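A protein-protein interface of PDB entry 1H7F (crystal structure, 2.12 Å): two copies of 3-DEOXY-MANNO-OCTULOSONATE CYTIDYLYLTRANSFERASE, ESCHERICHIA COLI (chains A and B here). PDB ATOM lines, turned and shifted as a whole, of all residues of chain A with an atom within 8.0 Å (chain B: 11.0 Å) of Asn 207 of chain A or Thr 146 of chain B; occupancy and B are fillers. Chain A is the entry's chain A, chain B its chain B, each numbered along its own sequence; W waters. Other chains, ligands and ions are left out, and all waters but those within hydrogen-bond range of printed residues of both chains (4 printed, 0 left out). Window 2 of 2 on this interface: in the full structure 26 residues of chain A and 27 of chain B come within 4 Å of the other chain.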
ATOM      1  N   LEU A 189      32.619 -17.054 -18.833  1.00  0.00           N
ATOM      2  CA  LEU A 189      31.715 -17.217 -17.694  1.00  0.00           C
ATOM      3  C   LEU A 189      30.717 -16.077 -17.601  1.00  0.00           C
ATOM      4  O   LEU A 189      31.080 -14.908 -17.715  1.00  0.00           O
ATOM      5  CB  LEU A 189      32.503 -17.302 -16.392  1.00  0.00           C
ATOM      6  CG  LEU A 189      33.444 -18.492 -16.237  1.00  0.00           C
ATOM      7  CD1 LEU A 189      34.122 -18.420 -14.890  1.00  0.00           C
ATOM      8  CD2 LEU A 189      32.671 -19.793 -16.387  1.00  0.00           C
ATOM      9  N   PRO A 190      29.426 -16.400 -17.440  1.00  0.00           N
ATOM     10  CA  PRO A 190      28.454 -15.308 -17.345  1.00  0.00           C
ATOM     11  C   PRO A 190      28.423 -14.741 -15.921  1.00  0.00           C
ATOM     12  O   PRO A 190      28.886 -15.394 -14.976  1.00  0.00           O
ATOM     13  CB  PRO A 190      27.140 -15.995 -17.725  1.00  0.00           C
ATOM     14  CG  PRO A 190      27.316 -17.387 -17.170  1.00  0.00           C
ATOM     15  CD  PRO A 190      28.765 -17.721 -17.473  1.00  0.00           C
ATOM     16  N   GLU A 191      27.981 -13.493 -15.786  1.00  0.00           N
ATOM     17  CA  GLU A 191      27.867 -12.868 -14.469  1.00  0.00           C
ATOM     18  C   GLU A 191      26.727 -13.578 -13.732  1.00  0.00           C
ATOM     19  O   GLU A 191      25.700 -13.897 -14.335  1.00  0.00           O
ATOM     20  CB  GLU A 191      27.507 -11.386 -14.596  1.00  0.00           C
ATOM     21  CG  GLU A 191      28.591 -10.492 -15.154  1.00  0.00           C
ATOM     22  CD  GLU A 191      28.151  -9.038 -15.213  1.00  0.00           C
ATOM     23  OE1 GLU A 191      27.750  -8.490 -14.164  1.00  0.00           O
ATOM     24  OE2 GLU A 191      28.191  -8.443 -16.309  1.00  0.00           O
ATOM     25  N   SER A 192      26.915 -13.850 -12.445  1.00  0.00           N
ATOM     26  CA  SER A 192      25.880 -14.515 -11.670  1.00  0.00           C
ATOM     27  C   SER A 192      25.031 -13.493 -10.932  1.00  0.00           C
ATOM     28  O   SER A 192      25.441 -12.340 -10.740  1.00  0.00           O
ATOM     29  CB  SER A 192      26.498 -15.481 -10.671  1.00  0.00           C
ATOM     30  OG  SER A 192      27.162 -14.779  -9.639  1.00  0.00           O
ATOM     31  N   MET A 193      23.843 -13.926 -10.512  1.00  0.00           N
ATOM     32  CA  MET A 193      22.925 -13.060  -9.781  1.00  0.00           C
ATOM     33  C   MET A 193      23.537 -12.690  -8.423  1.00  0.00           C
ATOM     34  O   MET A 193      23.516 -11.531  -8.040  1.00  0.00           O
ATOM     35  CB  MET A 193      21.545 -13.733  -9.651  1.00  0.00           C
ATOM     36  CG  MET A 193      20.494 -12.983  -8.812  1.00  0.00           C
ATOM     37  SD  MET A 193      20.771 -13.108  -7.036  1.00  0.00           S
ATOM     38  CE  MET A 193      20.493 -14.802  -6.811  1.00  0.00           C
ATOM     39  N   PRO A 194      24.119 -13.662  -7.692  1.00  0.00           N
ATOM     40  CA  PRO A 194      24.711 -13.305  -6.400  1.00  0.00           C
ATOM     41  C   PRO A 194      25.874 -12.320  -6.558  1.00  0.00           C
ATOM     42  O   PRO A 194      26.060 -11.431  -5.731  1.00  0.00           O
ATOM     43  CB  PRO A 194      25.190 -14.652  -5.864  1.00  0.00           C
ATOM     44  CG  PRO A 194      24.198 -15.593  -6.407  1.00  0.00           C
ATOM     45  CD  PRO A 194      24.073 -15.124  -7.842  1.00  0.00           C
ATOM     46  N   GLU A 195      26.646 -12.476  -7.633  1.00  0.00           N
ATOM     47  CA  GLU A 195      27.773 -11.590  -7.901  1.00  0.00           C
ATOM     48  C   GLU A 195      27.286 -10.166  -8.097  1.00  0.00           C
ATOM     49  O   GLU A 195      27.842  -9.234  -7.530  1.00  0.00           O
ATOM     50  CB  GLU A 195      28.520 -12.042  -9.160  1.00  0.00           C
ATOM     51  CG  GLU A 195      29.654 -11.088  -9.565  1.00  0.00           C
ATOM     52  CD  GLU A 195      30.016 -11.143 -11.038  1.00  0.00           C
ATOM     53  OE1 GLU A 195      29.699 -12.147 -11.709  1.00  0.00           O
ATOM     54  OE2 GLU A 195      30.623 -10.162 -11.519  1.00  0.00           O
ATOM     55  N   GLU A 201      33.066  -9.991  -7.260  1.00  0.00           N
ATOM     56  CA  GLU A 201      33.455 -10.698  -8.463  1.00  0.00           C
ATOM     57  C   GLU A 201      33.794 -12.167  -8.289  1.00  0.00           C
ATOM     58  O   GLU A 201      33.529 -12.967  -9.189  1.00  0.00           O
ATOM     59  CB  GLU A 201      34.604  -9.969  -9.140  1.00  0.00           C
ATOM     60  CG  GLU A 201      34.838 -10.420 -10.567  1.00  0.00           C
ATOM     61  CD  GLU A 201      35.942  -9.649 -11.272  1.00  0.00           C
ATOM     62  OE1 GLU A 201      36.739  -8.961 -10.590  1.00  0.00           O
ATOM     63  OE2 GLU A 201      36.011  -9.742 -12.520  1.00  0.00           O
ATOM     64  N   GLN A 202      34.312 -12.552  -7.126  1.00  0.00           N
ATOM     65  CA  GLN A 202      34.673 -13.951  -6.911  1.00  0.00           C
ATOM     66  C   GLN A 202      33.485 -14.918  -6.935  1.00  0.00           C
ATOM     67  O   GLN A 202      33.664 -16.132  -7.052  1.00  0.00           O
ATOM     68  CB  GLN A 202      35.488 -14.132  -5.622  1.00  0.00           C
ATOM     69  CG  GLN A 202      34.777 -13.783  -4.317  1.00  0.00           C
ATOM     70  CD  GLN A 202      34.891 -12.321  -3.936  1.00  0.00           C
ATOM     71  OE1 GLN A 202      34.658 -11.429  -4.749  1.00  0.00           O
ATOM     72  NE2 GLN A 202      35.236 -12.069  -2.684  1.00  0.00           N
ATOM     73  N   LEU A 203      32.269 -14.387  -6.843  1.00  0.00           N
ATOM     74  CA  LEU A 203      31.095 -15.247  -6.872  1.00  0.00           C
ATOM     75  C   LEU A 203      30.841 -15.742  -8.285  1.00  0.00           C
ATOM     76  O   LEU A 203      30.142 -16.741  -8.473  1.00  0.00           O
ATOM     77  CB  LEU A 203      29.869 -14.526  -6.309  1.00  0.00           C
ATOM     78  CG  LEU A 203      29.990 -14.269  -4.807  1.00  0.00           C
ATOM     79  CD1 LEU A 203      28.780 -13.497  -4.314  1.00  0.00           C
ATOM     80  CD2 LEU A 203      30.153 -15.593  -4.070  1.00  0.00           C
ATOM     81  N   ARG A 204      31.450 -15.084  -9.276  1.00  0.00           N
ATOM     82  CA  ARG A 204      31.284 -15.512 -10.668  1.00  0.00           C
ATOM     83  C   ARG A 204      31.906 -16.883 -10.847  1.00  0.00           C
ATOM     84  O   ARG A 204      31.399 -17.708 -11.606  1.00  0.00           O
ATOM     85  CB  ARG A 204      31.931 -14.540 -11.649  1.00  0.00           C
ATOM     86  CG  ARG A 204      31.665 -14.917 -13.096  1.00  0.00           C
ATOM     87  CD  ARG A 204      32.273 -13.928 -14.048  1.00  0.00           C
ATOM     88  NE  ARG A 204      31.829 -12.569 -13.774  1.00  0.00           N
ATOM     89  CZ  ARG A 204      32.274 -11.497 -14.417  1.00  0.00           C
ATOM     90  NH1 ARG A 204      33.174 -11.627 -15.382  1.00  0.00           N
ATOM     91  NH2 ARG A 204      31.856 -10.288 -14.067  1.00  0.00           N
ATOM     92  N   LEU A 205      32.976 -17.144 -10.106  1.00  0.00           N
ATOM     93  CA  LEU A 205      33.660 -18.424 -10.179  1.00  0.00           C
ATOM     94  C   LEU A 205      32.848 -19.510  -9.506  1.00  0.00           C
ATOM     95  O   LEU A 205      32.767 -20.640 -10.004  1.00  0.00           O
ATOM     96  CB  LEU A 205      35.033 -18.344  -9.506  1.00  0.00           C
ATOM     97  CG  LEU A 205      36.079 -17.426 -10.154  1.00  0.00           C
ATOM     98  CD1 LEU A 205      37.299 -17.305  -9.246  1.00  0.00           C
ATOM     99  CD2 LEU A 205      36.491 -17.993 -11.501  1.00  0.00           C
ATOM    100  N   MET A 206      32.283 -19.179  -8.344  1.00  0.00           N
ATOM    101  CA  MET A 206      31.482 -20.130  -7.587  1.00  0.00           C
ATOM    102  C   MET A 206      30.217 -20.528  -8.332  1.00  0.00           C
ATOM    103  O   MET A 206      29.770 -21.663  -8.240  1.00  0.00           O
ATOM    104  CB  MET A 206      31.156 -19.557  -6.214  1.00  0.00           C
ATOM    105  CG  MET A 206      32.400 -19.231  -5.419  1.00  0.00           C
ATOM    106  SD  MET A 206      32.028 -19.052  -3.700  1.00  0.00           S
ATOM    107  CE  MET A 206      32.243 -20.744  -3.166  1.00  0.00           C
ATOM    108  N   ASN A 207      29.653 -19.596  -9.087  1.00  0.00           N
ATOM    109  CA  ASN A 207      28.458 -19.866  -9.882  1.00  0.00           C
ATOM    110  C   ASN A 207      28.726 -20.959 -10.918  1.00  0.00           C
ATOM    111  O   ASN A 207      27.850 -21.783 -11.209  1.00  0.00           O
ATOM    112  CB  ASN A 207      28.025 -18.596 -10.603  1.00  0.00           C
ATOM    113  CG  ASN A 207      26.696 -18.754 -11.315  1.00  0.00           C
ATOM    114  OD1 ASN A 207      25.736 -19.242 -10.736  1.00  0.00           O
ATOM    115  ND2 ASN A 207      26.630 -18.317 -12.568  1.00  0.00           N
ATOM    116  N   ALA A 208      29.947 -20.961 -11.459  1.00  0.00           N
ATOM    117  CA  ALA A 208      30.371 -21.921 -12.482  1.00  0.00           C
ATOM    118  C   ALA A 208      30.920 -23.215 -11.901  1.00  0.00           C
ATOM    119  O   ALA A 208      31.409 -24.075 -12.628  1.00  0.00           O
ATOM    120  CB  ALA A 208      31.396 -21.282 -13.398  1.00  0.00           C
ATOM    121  N   GLY A 209      30.869 -23.342 -10.586  1.00  0.00           N
ATOM    122  CA  GLY A 209      31.335 -24.565  -9.955  1.00  0.00           C
ATOM    123  C   GLY A 209      32.828 -24.674  -9.774  1.00  0.00           C
ATOM    124  O   GLY A 209      33.348 -25.762  -9.509  1.00  0.00           O
ATOM    125  N   ILE A 210      33.527 -23.551  -9.884  1.00  0.00           N
ATOM    126  CA  ILE A 210      34.974 -23.561  -9.723  1.00  0.00           C
ATOM    127  C   ILE A 210      35.313 -23.424  -8.247  1.00  0.00           C
ATOM    128  O   ILE A 210      34.946 -22.450  -7.602  1.00  0.00           O
ATOM    129  CB  ILE A 210      35.619 -22.426 -10.542  1.00  0.00           C
ATOM    130  CG1 ILE A 210      35.340 -22.668 -12.030  1.00  0.00           C
ATOM    131  CG2 ILE A 210      37.122 -22.356 -10.271  1.00  0.00           C
ATOM    132  CD1 ILE A 210      35.577 -21.479 -12.912  1.00  0.00           C
ATOM    133  N   ILE A 212      37.283 -22.804  -4.795  1.00  0.00           N
ATOM    134  CA  ILE A 212      38.216 -21.803  -4.302  1.00  0.00           C
ATOM    135  C   ILE A 212      38.629 -22.227  -2.894  1.00  0.00           C
ATOM    136  O   ILE A 212      37.795 -22.251  -2.002  1.00  0.00           O
ATOM    137  CB  ILE A 212      37.548 -20.434  -4.207  1.00  0.00           C
ATOM    138  CG1 ILE A 212      37.036 -19.988  -5.573  1.00  0.00           C
ATOM    139  CG2 ILE A 212      38.514 -19.413  -3.631  1.00  0.00           C
ATOM    140  CD1 ILE A 212      36.306 -18.651  -5.544  1.00  0.00           C
ATOM    141  N   VAL B 143      21.349 -20.084  -1.473  1.00  0.00           N
ATOM    142  CA  VAL B 143      21.946 -19.502  -2.683  1.00  0.00           C
ATOM    143  C   VAL B 143      22.493 -20.688  -3.469  1.00  0.00           C
ATOM    144  O   VAL B 143      23.141 -21.572  -2.912  1.00  0.00           O
ATOM    145  CB  VAL B 143      23.093 -18.498  -2.368  1.00  0.00           C
ATOM    146  CG1 VAL B 143      23.801 -18.088  -3.643  1.00  0.00           C
ATOM    147  CG2 VAL B 143      22.534 -17.246  -1.733  1.00  0.00           C
ATOM    148  N   VAL B 144      22.190 -20.730  -4.758  1.00  0.00           N
ATOM    149  CA  VAL B 144      22.617 -21.844  -5.598  1.00  0.00           C
ATOM    150  C   VAL B 144      23.453 -21.402  -6.797  1.00  0.00           C
ATOM    151  O   VAL B 144      23.464 -20.227  -7.157  1.00  0.00           O
ATOM    152  CB  VAL B 144      21.376 -22.610  -6.145  1.00  0.00           C
ATOM    153  CG1 VAL B 144      20.477 -23.058  -4.996  1.00  0.00           C
ATOM    154  CG2 VAL B 144      20.580 -21.710  -7.113  1.00  0.00           C
ATOM    155  N   ASN B 145      24.132 -22.360  -7.420  1.00  0.00           N
ATOM    156  CA  ASN B 145      24.944 -22.081  -8.606  1.00  0.00           C
ATOM    157  C   ASN B 145      24.118 -22.422  -9.859  1.00  0.00           C
ATOM    158  O   ASN B 145      22.923 -22.698  -9.742  1.00  0.00           O
ATOM    159  CB  ASN B 145      26.277 -22.848  -8.547  1.00  0.00           C
ATOM    160  CG  ASN B 145      26.096 -24.343  -8.552  1.00  0.00           C
ATOM    161  OD1 ASN B 145      25.052 -24.852  -8.940  1.00  0.00           O
ATOM    162  ND2 ASN B 145      27.127 -25.061  -8.141  1.00  0.00           N
ATOM    163  N   THR B 146      24.722 -22.387 -11.048  1.00  0.00           N
ATOM    164  CA  THR B 146      23.985 -22.682 -12.286  1.00  0.00           C
ATOM    165  C   THR B 146      23.418 -24.097 -12.381  1.00  0.00           C
ATOM    166  O   THR B 146      22.443 -24.325 -13.088  1.00  0.00           O
ATOM    167  CB  THR B 146      24.816 -22.399 -13.559  1.00  0.00           C
ATOM    168  OG1 THR B 146      26.053 -23.108 -13.486  1.00  0.00           O
ATOM    169  CG2 THR B 146      25.087 -20.918 -13.706  1.00  0.00           C
ATOM    170  N   ARG B 147      24.057 -25.050 -11.716  1.00  0.00           N
ATOM    171  CA  ARG B 147      23.566 -26.426 -11.704  1.00  0.00           C
ATOM    172  C   ARG B 147      22.532 -26.611 -10.585  1.00  0.00           C
ATOM    173  O   ARG B 147      22.073 -27.723 -10.341  1.00  0.00           O
ATOM    174  CB  ARG B 147      24.707 -27.413 -11.478  1.00  0.00           C
ATOM    175  CG  ARG B 147      25.436 -27.841 -12.716  1.00  0.00           C
ATOM    176  CD  ARG B 147      26.452 -28.898 -12.338  1.00  0.00           C
ATOM    177  NE  ARG B 147      27.230 -29.344 -13.487  1.00  0.00           N
ATOM    178  CZ  ARG B 147      27.976 -30.444 -13.503  1.00  0.00           C
ATOM    179  NH1 ARG B 147      28.048 -31.218 -12.426  1.00  0.00           N
ATOM    180  NH2 ARG B 147      28.653 -30.767 -14.598  1.00  0.00           N
ATOM    181  N   GLN B 148      22.211 -25.523  -9.892  1.00  0.00           N
ATOM    182  CA  GLN B 148      21.246 -25.521  -8.797  1.00  0.00           C
ATOM    183  C   GLN B 148      21.756 -26.160  -7.516  1.00  0.00           C
ATOM    184  O   GLN B 148      20.978 -26.497  -6.624  1.00  0.00           O
ATOM    185  CB  GLN B 148      19.917 -26.146  -9.234  1.00  0.00           C
ATOM    186  CG  GLN B 148      19.223 -25.348 -10.318  1.00  0.00           C
ATOM    187  CD  GLN B 148      17.900 -25.949 -10.734  1.00  0.00           C
ATOM    188  OE1 GLN B 148      17.766 -27.166 -10.882  1.00  0.00           O
ATOM    189  NE2 GLN B 148      16.906 -25.090 -10.925  1.00  0.00           N
ATOM    190  N   ASP B 149      23.066 -26.346  -7.429  1.00  0.00           N
ATOM    191  CA  ASP B 149      23.665 -26.901  -6.230  1.00  0.00           C
ATOM    192  C   ASP B 149      23.702 -25.761  -5.228  1.00  0.00           C
ATOM    193  O   ASP B 149      23.911 -24.605  -5.600  1.00  0.00           O
ATOM    194  CB  ASP B 149      25.090 -27.379  -6.488  1.00  0.00           C
ATOM    195  CG  ASP B 149      25.152 -28.559  -7.420  1.00  0.00           C
ATOM    196  OD1 ASP B 149      24.218 -29.383  -7.423  1.00  0.00           O
ATOM    197  OD2 ASP B 149      26.163 -28.676  -8.142  1.00  0.00           O
ATOM    198  N   ALA B 150      23.466 -26.080  -3.962  1.00  0.00           N
ATOM    199  CA  ALA B 150      23.470 -25.058  -2.929  1.00  0.00           C
ATOM    200  C   ALA B 150      24.893 -24.658  -2.566  1.00  0.00           C
ATOM    201  O   ALA B 150      25.772 -25.510  -2.420  1.00  0.00           O
ATOM    202  CB  ALA B 150      22.741 -25.571  -1.684  1.00  0.00           C
ATOM    203  N   LEU B 151      25.114 -23.354  -2.446  1.00  0.00           N
ATOM    204  CA  LEU B 151      26.414 -22.844  -2.051  1.00  0.00           C
ATOM    205  C   LEU B 151      26.434 -22.720  -0.524  1.00  0.00           C
ATOM    206  O   LEU B 151      27.422 -23.078   0.126  1.00  0.00           O
ATOM    207  CB  LEU B 151      26.658 -21.479  -2.683  1.00  0.00           C
ATOM    208  CG  LEU B 151      26.816 -21.450  -4.204  1.00  0.00           C
ATOM    209  CD1 LEU B 151      26.963 -20.034  -4.674  1.00  0.00           C
ATOM    210  CD2 LEU B 151      28.017 -22.276  -4.593  1.00  0.00           C
ATOM    211  N   TYR B 152      25.325 -22.256   0.045  1.00  0.00           N
ATOM    212  CA  TYR B 152      25.221 -22.096   1.495  1.00  0.00           C
ATOM    213  C   TYR B 152      23.755 -21.884   1.880  1.00  0.00           C
ATOM    214  O   TYR B 152      22.943 -21.458   1.054  1.00  0.00           O
ATOM    215  CB  TYR B 152      26.070 -20.874   1.933  1.00  0.00           C
ATOM    216  CG  TYR B 152      26.254 -20.718   3.432  1.00  0.00           C
ATOM    217  CD1 TYR B 152      26.788 -21.749   4.198  1.00  0.00           C
ATOM    218  CD2 TYR B 152      25.863 -19.549   4.084  1.00  0.00           C
ATOM    219  CE1 TYR B 152      26.921 -21.621   5.575  1.00  0.00           C
ATOM    220  CE2 TYR B 152      25.994 -19.417   5.456  1.00  0.00           C
ATOM    221  CZ  TYR B 152      26.516 -20.454   6.194  1.00  0.00           C
ATOM    222  OH  TYR B 152      26.609 -20.338   7.563  1.00  0.00           O
ATOM    223  N   PRO B 159      21.539 -13.504  -1.076  1.00  0.00           N
ATOM    224  CA  PRO B 159      22.676 -12.580  -1.161  1.00  0.00           C
ATOM    225  C   PRO B 159      22.440 -11.198  -0.590  1.00  0.00           C
ATOM    226  O   PRO B 159      21.347 -10.643  -0.709  1.00  0.00           O
ATOM    227  CB  PRO B 159      22.920 -12.497  -2.666  1.00  0.00           C
ATOM    228  CG  PRO B 159      21.531 -12.597  -3.222  1.00  0.00           C
ATOM    229  CD  PRO B 159      20.970 -13.746  -2.416  1.00  0.00           C
ATOM    230  N   LEU B 170      15.610 -17.001  -2.228  1.00  0.00           N
ATOM    231  CA  LEU B 170      15.002 -18.319  -2.223  1.00  0.00           C
ATOM    232  C   LEU B 170      14.892 -18.825  -0.802  1.00  0.00           C
ATOM    233  O   LEU B 170      15.838 -18.725  -0.026  1.00  0.00           O
ATOM    234  CB  LEU B 170      15.846 -19.323  -3.015  1.00  0.00           C
ATOM    235  CG  LEU B 170      15.994 -19.085  -4.515  1.00  0.00           C
ATOM    236  CD1 LEU B 170      17.045 -20.019  -5.054  1.00  0.00           C
ATOM    237  CD2 LEU B 170      14.663 -19.294  -5.220  1.00  0.00           C
ATOM    238  N   ASN B 211      27.334 -32.760  -1.657  1.00  0.00           N
ATOM    239  CA  ASN B 211      26.542 -31.854  -2.463  1.00  0.00           C
ATOM    240  C   ASN B 211      25.049 -31.980  -2.196  1.00  0.00           C
ATOM    241  O   ASN B 211      24.532 -33.078  -2.008  1.00  0.00           O
ATOM    242  CB  ASN B 211      26.821 -32.116  -3.942  1.00  0.00           C
ATOM    243  CG  ASN B 211      26.185 -31.085  -4.838  1.00  0.00           C
ATOM    244  OD1 ASN B 211      26.332 -29.881  -4.615  1.00  0.00           O
ATOM    245  ND2 ASN B 211      25.463 -31.545  -5.860  1.00  0.00           N
ATOM    246  N   ILE B 212      24.357 -30.852  -2.256  1.00  0.00           N
ATOM    247  CA  ILE B 212      22.927 -30.806  -2.042  1.00  0.00           C
ATOM    248  C   ILE B 212      22.324 -30.022  -3.196  1.00  0.00           C
ATOM    249  O   ILE B 212      22.552 -28.827  -3.304  1.00  0.00           O
ATOM    250  CB  ILE B 212      22.583 -30.057  -0.700  1.00  0.00           C
ATOM    251  CG1 ILE B 212      23.116 -30.839   0.504  1.00  0.00           C
ATOM    252  CG2 ILE B 212      21.073 -29.858  -0.575  1.00  0.00           C
ATOM    253  CD1 ILE B 212      23.066 -30.049   1.809  1.00  0.00           C
ATOM    254  N   ARG B 213      21.589 -30.684  -4.086  1.00  0.00           N
ATOM    255  CA  ARG B 213      20.972 -29.955  -5.186  1.00  0.00           C
ATOM    256  C   ARG B 213      19.623 -29.448  -4.705  1.00  0.00           C
ATOM    257  O   ARG B 213      18.892 -30.156  -4.012  1.00  0.00           O
ATOM    258  CB  ARG B 213      20.829 -30.823  -6.444  1.00  0.00           C
ATOM    259  CG  ARG B 213      20.276 -30.059  -7.656  1.00  0.00           C
ATOM    260  CD  ARG B 213      20.736 -30.670  -8.966  1.00  0.00           C
ATOM    261  NE  ARG B 213      22.193 -30.699  -9.041  1.00  0.00           N
ATOM    262  CZ  ARG B 213      22.902 -31.716  -9.517  1.00  0.00           C
ATOM    263  NH1 ARG B 213      22.296 -32.798  -9.984  1.00  0.00           N
ATOM    264  NH2 ARG B 213      24.222 -31.682  -9.462  1.00  0.00           N
ATOM    265  N   THR B 214      19.292 -28.225  -5.093  1.00  0.00           N
ATOM    266  CA  THR B 214      18.062 -27.575  -4.681  1.00  0.00           C
ATOM    267  C   THR B 214      17.144 -27.242  -5.845  1.00  0.00           C
ATOM    268  O   THR B 214      17.465 -26.366  -6.635  1.00  0.00           O
ATOM    269  CB  THR B 214      18.404 -26.268  -3.945  1.00  0.00           C
ATOM    270  OG1 THR B 214      19.253 -26.561  -2.832  1.00  0.00           O
ATOM    271  CG2 THR B 214      17.167 -25.591  -3.431  1.00  0.00           C
ATOM    272  N   PHE B 215      15.989 -27.909  -5.911  1.00  0.00           N
ATOM    273  CA  PHE B 215      15.001 -27.693  -6.960  1.00  0.00           C
ATOM    274  C   PHE B 215      13.964 -26.677  -6.530  1.00  0.00           C
ATOM    275  O   PHE B 215      13.460 -26.733  -5.414  1.00  0.00           O
ATOM    276  CB  PHE B 215      14.306 -29.003  -7.322  1.00  0.00           C
ATOM    277  CG  PHE B 215      15.246 -30.073  -7.765  1.00  0.00           C
ATOM    278  CD1 PHE B 215      15.602 -30.192  -9.103  1.00  0.00           C
ATOM    279  CD2 PHE B 215      15.798 -30.953  -6.848  1.00  0.00           C
ATOM    280  CE1 PHE B 215      16.495 -31.172  -9.515  1.00  0.00           C
ATOM    281  CE2 PHE B 215      16.689 -31.932  -7.253  1.00  0.00           C
ATOM    282  CZ  PHE B 215      17.038 -32.041  -8.585  1.00  0.00           C
ATOM    283  N   GLU B 216      13.603 -25.789  -7.449  1.00  0.00           N
ATOM    284  CA  GLU B 216      12.650 -24.732  -7.173  1.00  0.00           C
ATOM    285  C   GLU B 216      11.209 -25.060  -7.528  1.00  0.00           C
ATOM    286  O   GLU B 216      10.915 -25.485  -8.645  1.00  0.00           O
ATOM    287  CB  GLU B 216      13.071 -23.460  -7.904  1.00  0.00           C
ATOM    288  CG  GLU B 216      12.177 -22.265  -7.622  1.00  0.00           C
ATOM    289  CD  GLU B 216      12.567 -21.026  -8.396  1.00  0.00           C
ATOM    290  OE1 GLU B 216      13.673 -20.998  -8.969  1.00  0.00           O
ATOM    291  OE2 GLU B 216      11.769 -20.071  -8.424  1.00  0.00           O
HETATM  292  O   HOH W   1      29.972 -23.844  -7.139  1.00  0.00           O
HETATM  293  O   HOH W   2      27.285 -24.733 -11.793  1.00  0.00           O
HETATM  294  O   HOH W   3      25.686 -18.670  -8.070  1.00  0.00           O
HETATM  295  O   HOH W   4      22.818 -19.465 -11.173  1.00  0.00           O
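Among the printed residues, merely in contact across the chains: Asn 207 of chain A with Asn 145 of chain B, Met 206 of chain A with Asn 145 of chain B, Pro 194 of chain A with Val 143 of chain B and Met 193 of chain A with Pro 159 of chain B.
The backbone carbonyl oxygen (O) of Asn 207 of chain A sits at hydrogen-bond distance from the side-chain hydroxyl (OG1) of Thr 146 of chain B, 3.2 Å away.
Position printed for both chains: 212. Of the 5 pairs that touch across the chains among the printed residues, none has its exchanged pair printed and touching as well.
Hydrophobic or aromatic side chains of chain A within 4 Å of the printed part of chain B: Met 193 and Pro 194. Along chain A the printed residues that touch a printed residue of chain B span positions 193 to 207. Hydrophobic or aromatic side chains of chain B within 4 Å of the printed part of chain A: Val 143 and Pro 159. Among the printed residues, 5 pairs touch across the chains. Among the printed residues, no Asp or Glu carboxylate lies within 4 Å of a Lys or Arg side-chain nitrogen of the other chain.
No residue of chain B comes within 4 Å of Ser 192 of chain A. Of the printed residues of chain B, Met 193 of chain A touches Pro 159 (3.9 Å). Met 206 of chain A touches just one residue of chain B: Asn 145 (3.7 Å). No residue of chain B comes within 4 Å of Ala 208 of chain A. Arg 147 of chain B touches none of the printed residues of chain A. Tyr 152 of chain B touches none of the printed residues of chain A. Of the printed residues of chain A, Pro 159 of chain B touches Met 193 (3.9 Å). The nearest residue of chain B that does not touch Asn 207 of chain A is Val 144 of chain B (4.4 Å).
N of Val 143 of chain B is in hydrogen-bond range of O of Tyr 152 of chain B. O of Val 143 of chain B is in hydrogen-bond range of N of Leu 151 of chain B (2.7 Å). The side-chain amide oxygen (OD1) of Asn 145 of chain B is in hydrogen-bond range of the backbone NH (N) of Arg 147 of chain B, 3.0 Å away. N of Asp 149 of chain B sits at hydrogen-bond distance from OD1 of Asn 145 of chain B (2.9 Å). The backbone NH (N) of Gln 148 of chain B lies within hydrogen-bond range of the side-chain amide oxygen (OD1) of Asn 145 of chain B (3.1 Å).
Water W1 lies within hydrogen-bond range of the backbone carbonyl oxygen of Met 206 of chain A and the side-chain amide nitrogen of Asn 145 of chain B. Water W2 lies within hydrogen-bond range of the side-chain hydroxyl of Thr 146 of chain B (2.7 Å), the backbone carbonyl oxygen of Asn 207 of chain A (3.1 Å) and the backbone NH of Arg 147 of chain B (3.2 Å). Water W3 lies within hydrogen-bond range of the side-chain amide oxygen of Asn 207 of chain A and the backbone carbonyl oxygen of Val 144 of chain B. Water W4 lies within hydrogen-bond range of OD1 of Asn 207 of chain A and N of Thr 146 of chain B.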
